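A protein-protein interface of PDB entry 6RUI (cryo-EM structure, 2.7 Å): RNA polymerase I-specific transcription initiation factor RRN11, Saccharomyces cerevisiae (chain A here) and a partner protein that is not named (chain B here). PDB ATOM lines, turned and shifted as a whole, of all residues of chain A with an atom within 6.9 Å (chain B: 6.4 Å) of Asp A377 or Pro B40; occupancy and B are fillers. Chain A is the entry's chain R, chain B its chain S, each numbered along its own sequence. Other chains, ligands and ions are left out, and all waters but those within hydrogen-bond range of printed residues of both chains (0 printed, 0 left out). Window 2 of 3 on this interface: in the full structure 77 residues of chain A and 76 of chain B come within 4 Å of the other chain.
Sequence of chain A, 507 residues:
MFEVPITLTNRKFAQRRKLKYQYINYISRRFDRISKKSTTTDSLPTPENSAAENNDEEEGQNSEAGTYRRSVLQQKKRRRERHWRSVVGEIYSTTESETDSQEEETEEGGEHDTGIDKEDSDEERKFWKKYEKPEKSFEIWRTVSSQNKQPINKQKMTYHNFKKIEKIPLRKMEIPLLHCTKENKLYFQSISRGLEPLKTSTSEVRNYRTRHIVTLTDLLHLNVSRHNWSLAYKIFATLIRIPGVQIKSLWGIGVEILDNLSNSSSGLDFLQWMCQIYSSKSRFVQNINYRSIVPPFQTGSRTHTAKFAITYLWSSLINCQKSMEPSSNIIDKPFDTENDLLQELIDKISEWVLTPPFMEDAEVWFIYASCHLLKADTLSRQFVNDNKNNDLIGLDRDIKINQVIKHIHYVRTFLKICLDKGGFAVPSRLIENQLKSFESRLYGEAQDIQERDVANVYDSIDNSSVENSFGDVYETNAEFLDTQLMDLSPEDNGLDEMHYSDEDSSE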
ATOM      1  N   GLN A 321      -7.910 -14.914  36.261  1.00  0.00           N
ATOM      2  CA  GLN A 321      -6.723 -15.273  35.498  1.00  0.00           C
ATOM      3  C   GLN A 321      -5.545 -15.561  36.416  1.00  0.00           C
ATOM      4  O   GLN A 321      -4.852 -16.571  36.257  1.00  0.00           O
ATOM      5  CB  GLN A 321      -6.367 -14.149  34.540  1.00  0.00           C
ATOM      6  CG  GLN A 321      -5.141 -14.421  33.726  1.00  0.00           C
ATOM      7  CD  GLN A 321      -4.770 -13.254  32.855  1.00  0.00           C
ATOM      8  OE1 GLN A 321      -5.363 -12.178  32.936  1.00  0.00           O
ATOM      9  NE2 GLN A 321      -3.792 -13.462  31.994  1.00  0.00           N
ATOM     10  N   HIS A 372     -14.461 -15.392  27.319  1.00  0.00           N
ATOM     11  CA  HIS A 372     -14.382 -16.577  26.481  1.00  0.00           C
ATOM     12  C   HIS A 372     -13.049 -16.683  25.776  1.00  0.00           C
ATOM     13  O   HIS A 372     -12.616 -17.791  25.453  1.00  0.00           O
ATOM     14  CB  HIS A 372     -15.498 -16.592  25.447  1.00  0.00           C
ATOM     15  CG  HIS A 372     -16.852 -16.815  26.029  1.00  0.00           C
ATOM     16  ND1 HIS A 372     -17.213 -18.002  26.626  1.00  0.00           N
ATOM     17  CD2 HIS A 372     -17.949 -16.027  26.063  1.00  0.00           C
ATOM     18  CE1 HIS A 372     -18.463 -17.920  27.036  1.00  0.00           C
ATOM     19  NE2 HIS A 372     -18.936 -16.736  26.699  1.00  0.00           N
ATOM     20  N   LEU A 373     -12.384 -15.555  25.534  1.00  0.00           N
ATOM     21  CA  LEU A 373     -11.053 -15.601  24.947  1.00  0.00           C
ATOM     22  C   LEU A 373     -10.056 -16.195  25.922  1.00  0.00           C
ATOM     23  O   LEU A 373      -9.050 -16.768  25.501  1.00  0.00           O
ATOM     24  CB  LEU A 373     -10.620 -14.201  24.514  1.00  0.00           C
ATOM     25  CG  LEU A 373      -9.407 -14.018  23.597  1.00  0.00           C
ATOM     26  CD1 LEU A 373      -9.631 -12.816  22.712  1.00  0.00           C
ATOM     27  CD2 LEU A 373      -8.118 -13.818  24.348  1.00  0.00           C
ATOM     28  N   LEU A 374     -10.326 -16.089  27.217  1.00  0.00           N
ATOM     29  CA  LEU A 374      -9.391 -16.616  28.193  1.00  0.00           C
ATOM     30  C   LEU A 374      -9.540 -18.128  28.311  1.00  0.00           C
ATOM     31  O   LEU A 374      -8.546 -18.834  28.502  1.00  0.00           O
ATOM     32  CB  LEU A 374      -9.602 -15.915  29.534  1.00  0.00           C
ATOM     33  CG  LEU A 374      -8.388 -15.813  30.457  1.00  0.00           C
ATOM     34  CD1 LEU A 374      -8.514 -14.581  31.316  1.00  0.00           C
ATOM     35  CD2 LEU A 374      -8.195 -17.009  31.320  1.00  0.00           C
ATOM     36  N   LYS A 375     -10.768 -18.641  28.193  1.00  0.00           N
ATOM     37  CA  LYS A 375     -10.957 -20.085  28.102  1.00  0.00           C
ATOM     38  C   LYS A 375     -10.390 -20.620  26.798  1.00  0.00           C
ATOM     39  O   LYS A 375      -9.740 -21.670  26.782  1.00  0.00           O
ATOM     40  CB  LYS A 375     -12.439 -20.445  28.214  1.00  0.00           C
ATOM     41  CG  LYS A 375     -13.084 -20.073  29.527  1.00  0.00           C
ATOM     42  CD  LYS A 375     -12.532 -20.885  30.676  1.00  0.00           C
ATOM     43  CE  LYS A 375     -13.072 -22.304  30.717  1.00  0.00           C
ATOM     44  NZ  LYS A 375     -14.511 -22.341  31.096  1.00  0.00           N
ATOM     45  N   ALA A 376     -10.600 -19.896  25.697  1.00  0.00           N
ATOM     46  CA  ALA A 376     -10.042 -20.299  24.415  1.00  0.00           C
ATOM     47  C   ALA A 376      -8.526 -20.191  24.380  1.00  0.00           C
ATOM     48  O   ALA A 376      -7.894 -20.831  23.540  1.00  0.00           O
ATOM     49  CB  ALA A 376     -10.642 -19.451  23.299  1.00  0.00           C
ATOM     50  N   ASP A 377      -7.937 -19.394  25.266  1.00  0.00           N
ATOM     51  CA  ASP A 377      -6.489 -19.350  25.416  1.00  0.00           C
ATOM     52  C   ASP A 377      -5.986 -20.523  26.243  1.00  0.00           C
ATOM     53  O   ASP A 377      -4.993 -21.163  25.883  1.00  0.00           O
ATOM     54  CB  ASP A 377      -6.085 -18.050  26.094  1.00  0.00           C
ATOM     55  CG  ASP A 377      -4.601 -17.825  26.098  1.00  0.00           C
ATOM     56  OD1 ASP A 377      -3.859 -18.528  25.385  1.00  0.00           O
ATOM     57  OD2 ASP A 377      -4.171 -16.969  26.889  1.00  0.00           O
ATOM     58  N   THR A 378      -6.639 -20.782  27.377  1.00  0.00           N
ATOM     59  CA  THR A 378      -6.154 -21.783  28.318  1.00  0.00           C
ATOM     60  C   THR A 378      -6.290 -23.185  27.751  1.00  0.00           C
ATOM     61  O   THR A 378      -5.351 -23.985  27.819  1.00  0.00           O
ATOM     62  CB  THR A 378      -6.919 -21.653  29.635  1.00  0.00           C
ATOM     63  OG1 THR A 378      -6.645 -20.376  30.219  1.00  0.00           O
ATOM     64  CG2 THR A 378      -6.540 -22.748  30.614  1.00  0.00           C
ATOM     65  N   LEU A 379      -7.434 -23.481  27.143  1.00  0.00           N
ATOM     66  CA  LEU A 379      -7.696 -24.825  26.651  1.00  0.00           C
ATOM     67  C   LEU A 379      -6.913 -25.139  25.383  1.00  0.00           C
ATOM     68  O   LEU A 379      -6.804 -26.311  25.013  1.00  0.00           O
ATOM     69  CB  LEU A 379      -9.193 -25.005  26.397  1.00  0.00           C
ATOM     70  CG  LEU A 379     -10.110 -25.393  27.562  1.00  0.00           C
ATOM     71  CD1 LEU A 379      -9.652 -26.697  28.178  1.00  0.00           C
ATOM     72  CD2 LEU A 379     -10.265 -24.326  28.631  1.00  0.00           C
ATOM     73  N   SER A 380      -6.359 -24.127  24.722  1.00  0.00           N
ATOM     74  CA  SER A 380      -5.605 -24.325  23.487  1.00  0.00           C
ATOM     75  C   SER A 380      -4.127 -24.567  23.793  1.00  0.00           C
ATOM     76  O   SER A 380      -3.236 -23.808  23.418  1.00  0.00           O
ATOM     77  CB  SER A 380      -5.797 -23.133  22.559  1.00  0.00           C
ATOM     78  OG  SER A 380      -5.076 -23.293  21.350  1.00  0.00           O
ATOM     79  N   ARG A 381      -3.893 -25.628  24.516  1.00  0.00           N
ATOM     80  CA  ARG A 381      -2.582 -26.209  24.770  1.00  0.00           C
ATOM     81  C   ARG A 381      -2.556 -27.698  24.457  1.00  0.00           C
ATOM     82  O   ARG A 381      -1.496 -28.236  24.114  1.00  0.00           O
ATOM     83  CB  ARG A 381      -2.187 -25.957  26.227  1.00  0.00           C
ATOM     84  CG  ARG A 381      -2.051 -24.483  26.594  1.00  0.00           C
ATOM     85  CD  ARG A 381      -0.903 -23.851  25.825  1.00  0.00           C
ATOM     86  NE  ARG A 381      -0.579 -22.499  26.274  1.00  0.00           N
ATOM     87  CZ  ARG A 381       0.353 -21.734  25.709  1.00  0.00           C
ATOM     88  NH1 ARG A 381       0.598 -20.520  26.180  1.00  0.00           N
ATOM     89  NH2 ARG A 381       1.039 -22.182  24.665  1.00  0.00           N
ATOM     90  N   VAL A 404     -13.484 -25.691  22.266  1.00  0.00           N
ATOM     91  CA  VAL A 404     -12.700 -24.497  21.982  1.00  0.00           C
ATOM     92  C   VAL A 404     -13.325 -23.715  20.835  1.00  0.00           C
ATOM     93  O   VAL A 404     -13.358 -22.480  20.859  1.00  0.00           O
ATOM     94  CB  VAL A 404     -11.239 -24.883  21.694  1.00  0.00           C
ATOM     95  CG1 VAL A 404     -10.387 -23.656  21.392  1.00  0.00           C
ATOM     96  CG2 VAL A 404     -10.663 -25.641  22.865  1.00  0.00           C
ATOM     97  N   HIS A 407     -15.985 -21.524  22.195  1.00  0.00           N
ATOM     98  CA  HIS A 407     -15.476 -20.299  22.798  1.00  0.00           C
ATOM     99  C   HIS A 407     -14.933 -19.336  21.755  1.00  0.00           C
ATOM    100  O   HIS A 407     -15.060 -18.121  21.920  1.00  0.00           O
ATOM    101  CB  HIS A 407     -14.412 -20.629  23.832  1.00  0.00           C
ATOM    102  CG  HIS A 407     -14.960 -21.291  25.050  1.00  0.00           C
ATOM    103  ND1 HIS A 407     -15.088 -22.656  25.158  1.00  0.00           N
ATOM    104  CD2 HIS A 407     -15.435 -20.775  26.204  1.00  0.00           C
ATOM    105  CE1 HIS A 407     -15.606 -22.954  26.336  1.00  0.00           C
ATOM    106  NE2 HIS A 407     -15.826 -21.829  26.989  1.00  0.00           N
ATOM    107  N   ILE A 408     -14.323 -19.851  20.683  1.00  0.00           N
ATOM    108  CA  ILE A 408     -13.893 -18.986  19.584  1.00  0.00           C
ATOM    109  C   ILE A 408     -15.100 -18.332  18.924  1.00  0.00           C
ATOM    110  O   ILE A 408     -15.084 -17.135  18.607  1.00  0.00           O
ATOM    111  CB  ILE A 408     -13.047 -19.779  18.568  1.00  0.00           C
ATOM    112  CG1 ILE A 408     -11.729 -20.248  19.184  1.00  0.00           C
ATOM    113  CG2 ILE A 408     -12.736 -18.948  17.340  1.00  0.00           C
ATOM    114  CD1 ILE A 408     -10.795 -19.144  19.563  1.00  0.00           C
ATOM    115  N   GLN A 434      -5.187 -13.270  17.291  1.00  0.00           N
ATOM    116  CA  GLN A 434      -5.070 -14.163  18.432  1.00  0.00           C
ATOM    117  C   GLN A 434      -6.076 -15.298  18.409  1.00  0.00           C
ATOM    118  O   GLN A 434      -5.806 -16.356  18.984  1.00  0.00           O
ATOM    119  CB  GLN A 434      -5.232 -13.385  19.734  1.00  0.00           C
ATOM    120  CG  GLN A 434      -4.148 -12.371  19.937  1.00  0.00           C
ATOM    121  CD  GLN A 434      -2.776 -13.006  19.888  1.00  0.00           C
ATOM    122  OE1 GLN A 434      -2.027 -12.820  18.928  1.00  0.00           O
ATOM    123  NE2 GLN A 434      -2.438 -13.763  20.918  1.00  0.00           N
ATOM    124  N   PHE A 438      -5.223 -19.430  18.131  1.00  0.00           N
ATOM    125  CA  PHE A 438      -5.747 -20.485  18.986  1.00  0.00           C
ATOM    126  C   PHE A 438      -6.100 -21.716  18.171  1.00  0.00           C
ATOM    127  O   PHE A 438      -5.977 -22.844  18.659  1.00  0.00           O
ATOM    128  CB  PHE A 438      -6.972 -19.976  19.741  1.00  0.00           C
ATOM    129  CG  PHE A 438      -6.658 -18.930  20.763  1.00  0.00           C
ATOM    130  CD1 PHE A 438      -5.396 -18.846  21.327  1.00  0.00           C
ATOM    131  CD2 PHE A 438      -7.610 -17.998  21.125  1.00  0.00           C
ATOM    132  CE1 PHE A 438      -5.103 -17.876  22.257  1.00  0.00           C
ATOM    133  CE2 PHE A 438      -7.319 -17.022  22.052  1.00  0.00           C
ATOM    134  CZ  PHE A 438      -6.062 -16.962  22.617  1.00  0.00           C
ATOM    135  N   ARG A 441      -2.872 -23.718  16.746  1.00  0.00           N
ATOM    136  CA  ARG A 441      -2.425 -24.638  17.784  1.00  0.00           C
ATOM    137  C   ARG A 441      -3.362 -25.831  17.903  1.00  0.00           C
ATOM    138  O   ARG A 441      -3.000 -26.849  18.504  1.00  0.00           O
ATOM    139  CB  ARG A 441      -2.340 -23.896  19.114  1.00  0.00           C
ATOM    140  CG  ARG A 441      -1.282 -22.813  19.139  1.00  0.00           C
ATOM    141  CD  ARG A 441      -1.311 -22.035  20.443  1.00  0.00           C
ATOM    142  NE  ARG A 441      -0.245 -21.036  20.504  1.00  0.00           N
ATOM    143  CZ  ARG A 441      -0.086 -20.170  21.501  1.00  0.00           C
ATOM    144  NH1 ARG A 441       0.916 -19.304  21.474  1.00  0.00           N
ATOM    145  NH2 ARG A 441      -0.931 -20.165  22.522  1.00  0.00           N
ATOM    146  N   GLN B  37      -5.840  -6.053  27.273  1.00  0.00           N
ATOM    147  CA  GLN B  37      -5.748  -6.678  25.964  1.00  0.00           C
ATOM    148  C   GLN B  37      -5.832  -8.186  26.007  1.00  0.00           C
ATOM    149  O   GLN B  37      -6.305  -8.785  25.032  1.00  0.00           O
ATOM    150  CB  GLN B  37      -4.447  -6.295  25.271  1.00  0.00           C
ATOM    151  CG  GLN B  37      -4.515  -4.963  24.625  1.00  0.00           C
ATOM    152  CD  GLN B  37      -5.396  -5.019  23.431  1.00  0.00           C
ATOM    153  OE1 GLN B  37      -6.550  -4.606  23.477  1.00  0.00           O
ATOM    154  NE2 GLN B  37      -4.860  -5.528  22.332  1.00  0.00           N
ATOM    155  N   GLU B  38      -5.406  -8.795  27.113  1.00  0.00           N
ATOM    156  CA  GLU B  38      -5.103 -10.224  27.195  1.00  0.00           C
ATOM    157  C   GLU B  38      -4.110 -10.604  26.094  1.00  0.00           C
ATOM    158  O   GLU B  38      -4.450 -11.133  25.039  1.00  0.00           O
ATOM    159  CB  GLU B  38      -6.375 -11.090  27.210  1.00  0.00           C
ATOM    160  CG  GLU B  38      -6.172 -12.615  27.244  1.00  0.00           C
ATOM    161  CD  GLU B  38      -5.368 -13.117  28.416  1.00  0.00           C
ATOM    162  OE1 GLU B  38      -5.349 -12.464  29.476  1.00  0.00           O
ATOM    163  OE2 GLU B  38      -4.748 -14.187  28.276  1.00  0.00           O
ATOM    164  N   LYS B  39      -2.892 -10.138  26.318  1.00  0.00           N
ATOM    165  CA  LYS B  39      -1.727 -10.523  25.542  1.00  0.00           C
ATOM    166  C   LYS B  39      -1.149 -11.800  26.134  1.00  0.00           C
ATOM    167  O   LYS B  39      -0.446 -11.740  27.144  1.00  0.00           O
ATOM    168  CB  LYS B  39      -0.683  -9.410  25.563  1.00  0.00           C
ATOM    169  CG  LYS B  39      -1.152  -8.081  24.987  1.00  0.00           C
ATOM    170  CD  LYS B  39      -1.278  -8.151  23.478  1.00  0.00           C
ATOM    171  CE  LYS B  39      -1.691  -6.819  22.889  1.00  0.00           C
ATOM    172  NZ  LYS B  39      -0.633  -5.789  23.049  1.00  0.00           N
ATOM    173  N   PRO B  40      -1.395 -12.959  25.541  1.00  0.00           N
ATOM    174  CA  PRO B  40      -0.943 -14.224  26.151  1.00  0.00           C
ATOM    175  C   PRO B  40       0.534 -14.497  25.895  1.00  0.00           C
ATOM    176  O   PRO B  40       0.934 -15.406  25.159  1.00  0.00           O
ATOM    177  CB  PRO B  40      -1.849 -15.248  25.470  1.00  0.00           C
ATOM    178  CG  PRO B  40      -2.082 -14.676  24.126  1.00  0.00           C
ATOM    179  CD  PRO B  40      -2.113 -13.190  24.278  1.00  0.00           C
ATOM    180  N   GLN B  41       1.399 -13.713  26.534  1.00  0.00           N
ATOM    181  CA  GLN B  41       2.812 -13.747  26.187  1.00  0.00           C
ATOM    182  C   GLN B  41       3.713 -14.054  27.380  1.00  0.00           C
ATOM    183  O   GLN B  41       4.930 -13.845  27.285  1.00  0.00           O
ATOM    184  CB  GLN B  41       3.227 -12.424  25.537  1.00  0.00           C
ATOM    185  CG  GLN B  41       3.116 -11.229  26.462  1.00  0.00           C
ATOM    186  CD  GLN B  41       3.485  -9.935  25.787  1.00  0.00           C
ATOM    187  OE1 GLN B  41       3.850  -9.918  24.614  1.00  0.00           O
ATOM    188  NE2 GLN B  41       3.401  -8.838  26.527  1.00  0.00           N
ATOM    189  N   TRP B  42       3.142 -14.541  28.494  1.00  0.00           N
ATOM    190  CA  TRP B  42       3.860 -14.939  29.715  1.00  0.00           C
ATOM    191  C   TRP B  42       4.723 -13.817  30.291  1.00  0.00           C
ATOM    192  O   TRP B  42       5.746 -14.078  30.933  1.00  0.00           O
ATOM    193  CB  TRP B  42       4.728 -16.184  29.485  1.00  0.00           C
ATOM    194  CG  TRP B  42       3.967 -17.447  29.240  1.00  0.00           C
ATOM    195  CD1 TRP B  42       3.686 -18.013  28.032  1.00  0.00           C
ATOM    196  CD2 TRP B  42       3.405 -18.314  30.230  1.00  0.00           C
ATOM    197  NE1 TRP B  42       2.980 -19.176  28.207  1.00  0.00           N
ATOM    198  CE2 TRP B  42       2.793 -19.383  29.548  1.00  0.00           C
ATOM    199  CE3 TRP B  42       3.358 -18.289  31.628  1.00  0.00           C
ATOM    200  CZ2 TRP B  42       2.138 -20.420  30.217  1.00  0.00           C
ATOM    201  CZ3 TRP B  42       2.706 -19.318  32.291  1.00  0.00           C
ATOM    202  CH2 TRP B  42       2.107 -20.369  31.584  1.00  0.00           C
ATOM    203  N   LEU B  43       4.332 -12.571  30.053  1.00  0.00           N
ATOM    204  CA  LEU B  43       5.156 -11.403  30.325  1.00  0.00           C
ATOM    205  C   LEU B  43       4.276 -10.365  31.012  1.00  0.00           C
ATOM    206  O   LEU B  43       4.096  -9.249  30.525  1.00  0.00           O
ATOM    207  CB  LEU B  43       5.800 -10.906  29.026  1.00  0.00           C
ATOM    208  CG  LEU B  43       7.064 -10.036  28.991  1.00  0.00           C
ATOM    209  CD1 LEU B  43       7.859 -10.428  27.769  1.00  0.00           C
ATOM    210  CD2 LEU B  43       6.795  -8.540  28.943  1.00  0.00           C
ATOM    211  N   PRO B  45       0.655 -11.042  31.520  1.00  0.00           N
ATOM    212  CA  PRO B  45      -0.252 -11.071  30.360  1.00  0.00           C
ATOM    213  C   PRO B  45      -1.486 -10.184  30.473  1.00  0.00           C
ATOM    214  O   PRO B  45      -2.621 -10.667  30.463  1.00  0.00           O
ATOM    215  CB  PRO B  45      -0.643 -12.552  30.283  1.00  0.00           C
ATOM    216  CG  PRO B  45      -0.496 -13.055  31.669  1.00  0.00           C
ATOM    217  CD  PRO B  45       0.631 -12.307  32.280  1.00  0.00           C
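Of the 8 printed residues of chain B, 4 touch a printed residue of chain A.
Printed residues of chain B that touch a printed residue of chain A: Glu B38, Pro B40, Trp B42 and Pro B45.
Hydrophobic or aromatic side chains of chain B that line the printed part of chain A: Pro B40, Trp B42 and Pro B45.
Of the 17 printed residues of chain A, 5 touch a printed residue of chain B.
Hydrophobic or aromatic side chains of chain A that line the printed part of chain B: Leu A373.
Among the printed residues, 7 pairs touch across the chains.
Among the printed residues, no Asp or Glu carboxylate lies within 4 Å of a Lys or Arg side-chain nitrogen of the other chain.
OE1 of Glu B38 lies within hydrogen-bond range of NE2 of Gln A321 (3.1 Å).
The backbone carbonyl oxygen (O) of Pro B45 sits close to the side-chain amide nitrogen (NE2) of Gln A321 (3.4 Å).
The side-chain carboxylate (OE2) of Glu B38 sits close to the side-chain carboxylate (OD2) of Asp A377 (3.2 Å).
The guanidinium group (NH1) of Arg A381 sits close to the indole nitrogen (NE1) of Trp B42, at 3.4 Å.
Leu A373 touches Glu B38.
Pro B40 touches Asp A377 (CB to OD2, 3.2 Å).
Gln A434 touches Pro B40 (NE2 to CG, 3.4 Å).
Asp A377 touches two residues of chain B.
Of the printed residues of chain A, Pro B40 touches Asp A377 (3.2 Å) and Gln A434 (3.4 Å).
Printed residues of chain A within 4 Å of Pro B45: Gln A321.
Printed residues of chain A within 4 Å of Glu B38: Gln A321 (3.1 Å), Leu A373 (3.7 Å) and Asp A377 (3.2 Å).
Printed residues of chain B within 4 Å of Gln A434: Pro B40.
Of the printed residues of chain B, Gln A321 touches Glu B38 and Pro B45.
Ser A380 touches none of the printed residues of chain B.
Arg A441 touches none of the printed residues of chain B.
The nearest residue of chain B that does not touch Asp A377 is Lys B39 (6.0 Å).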
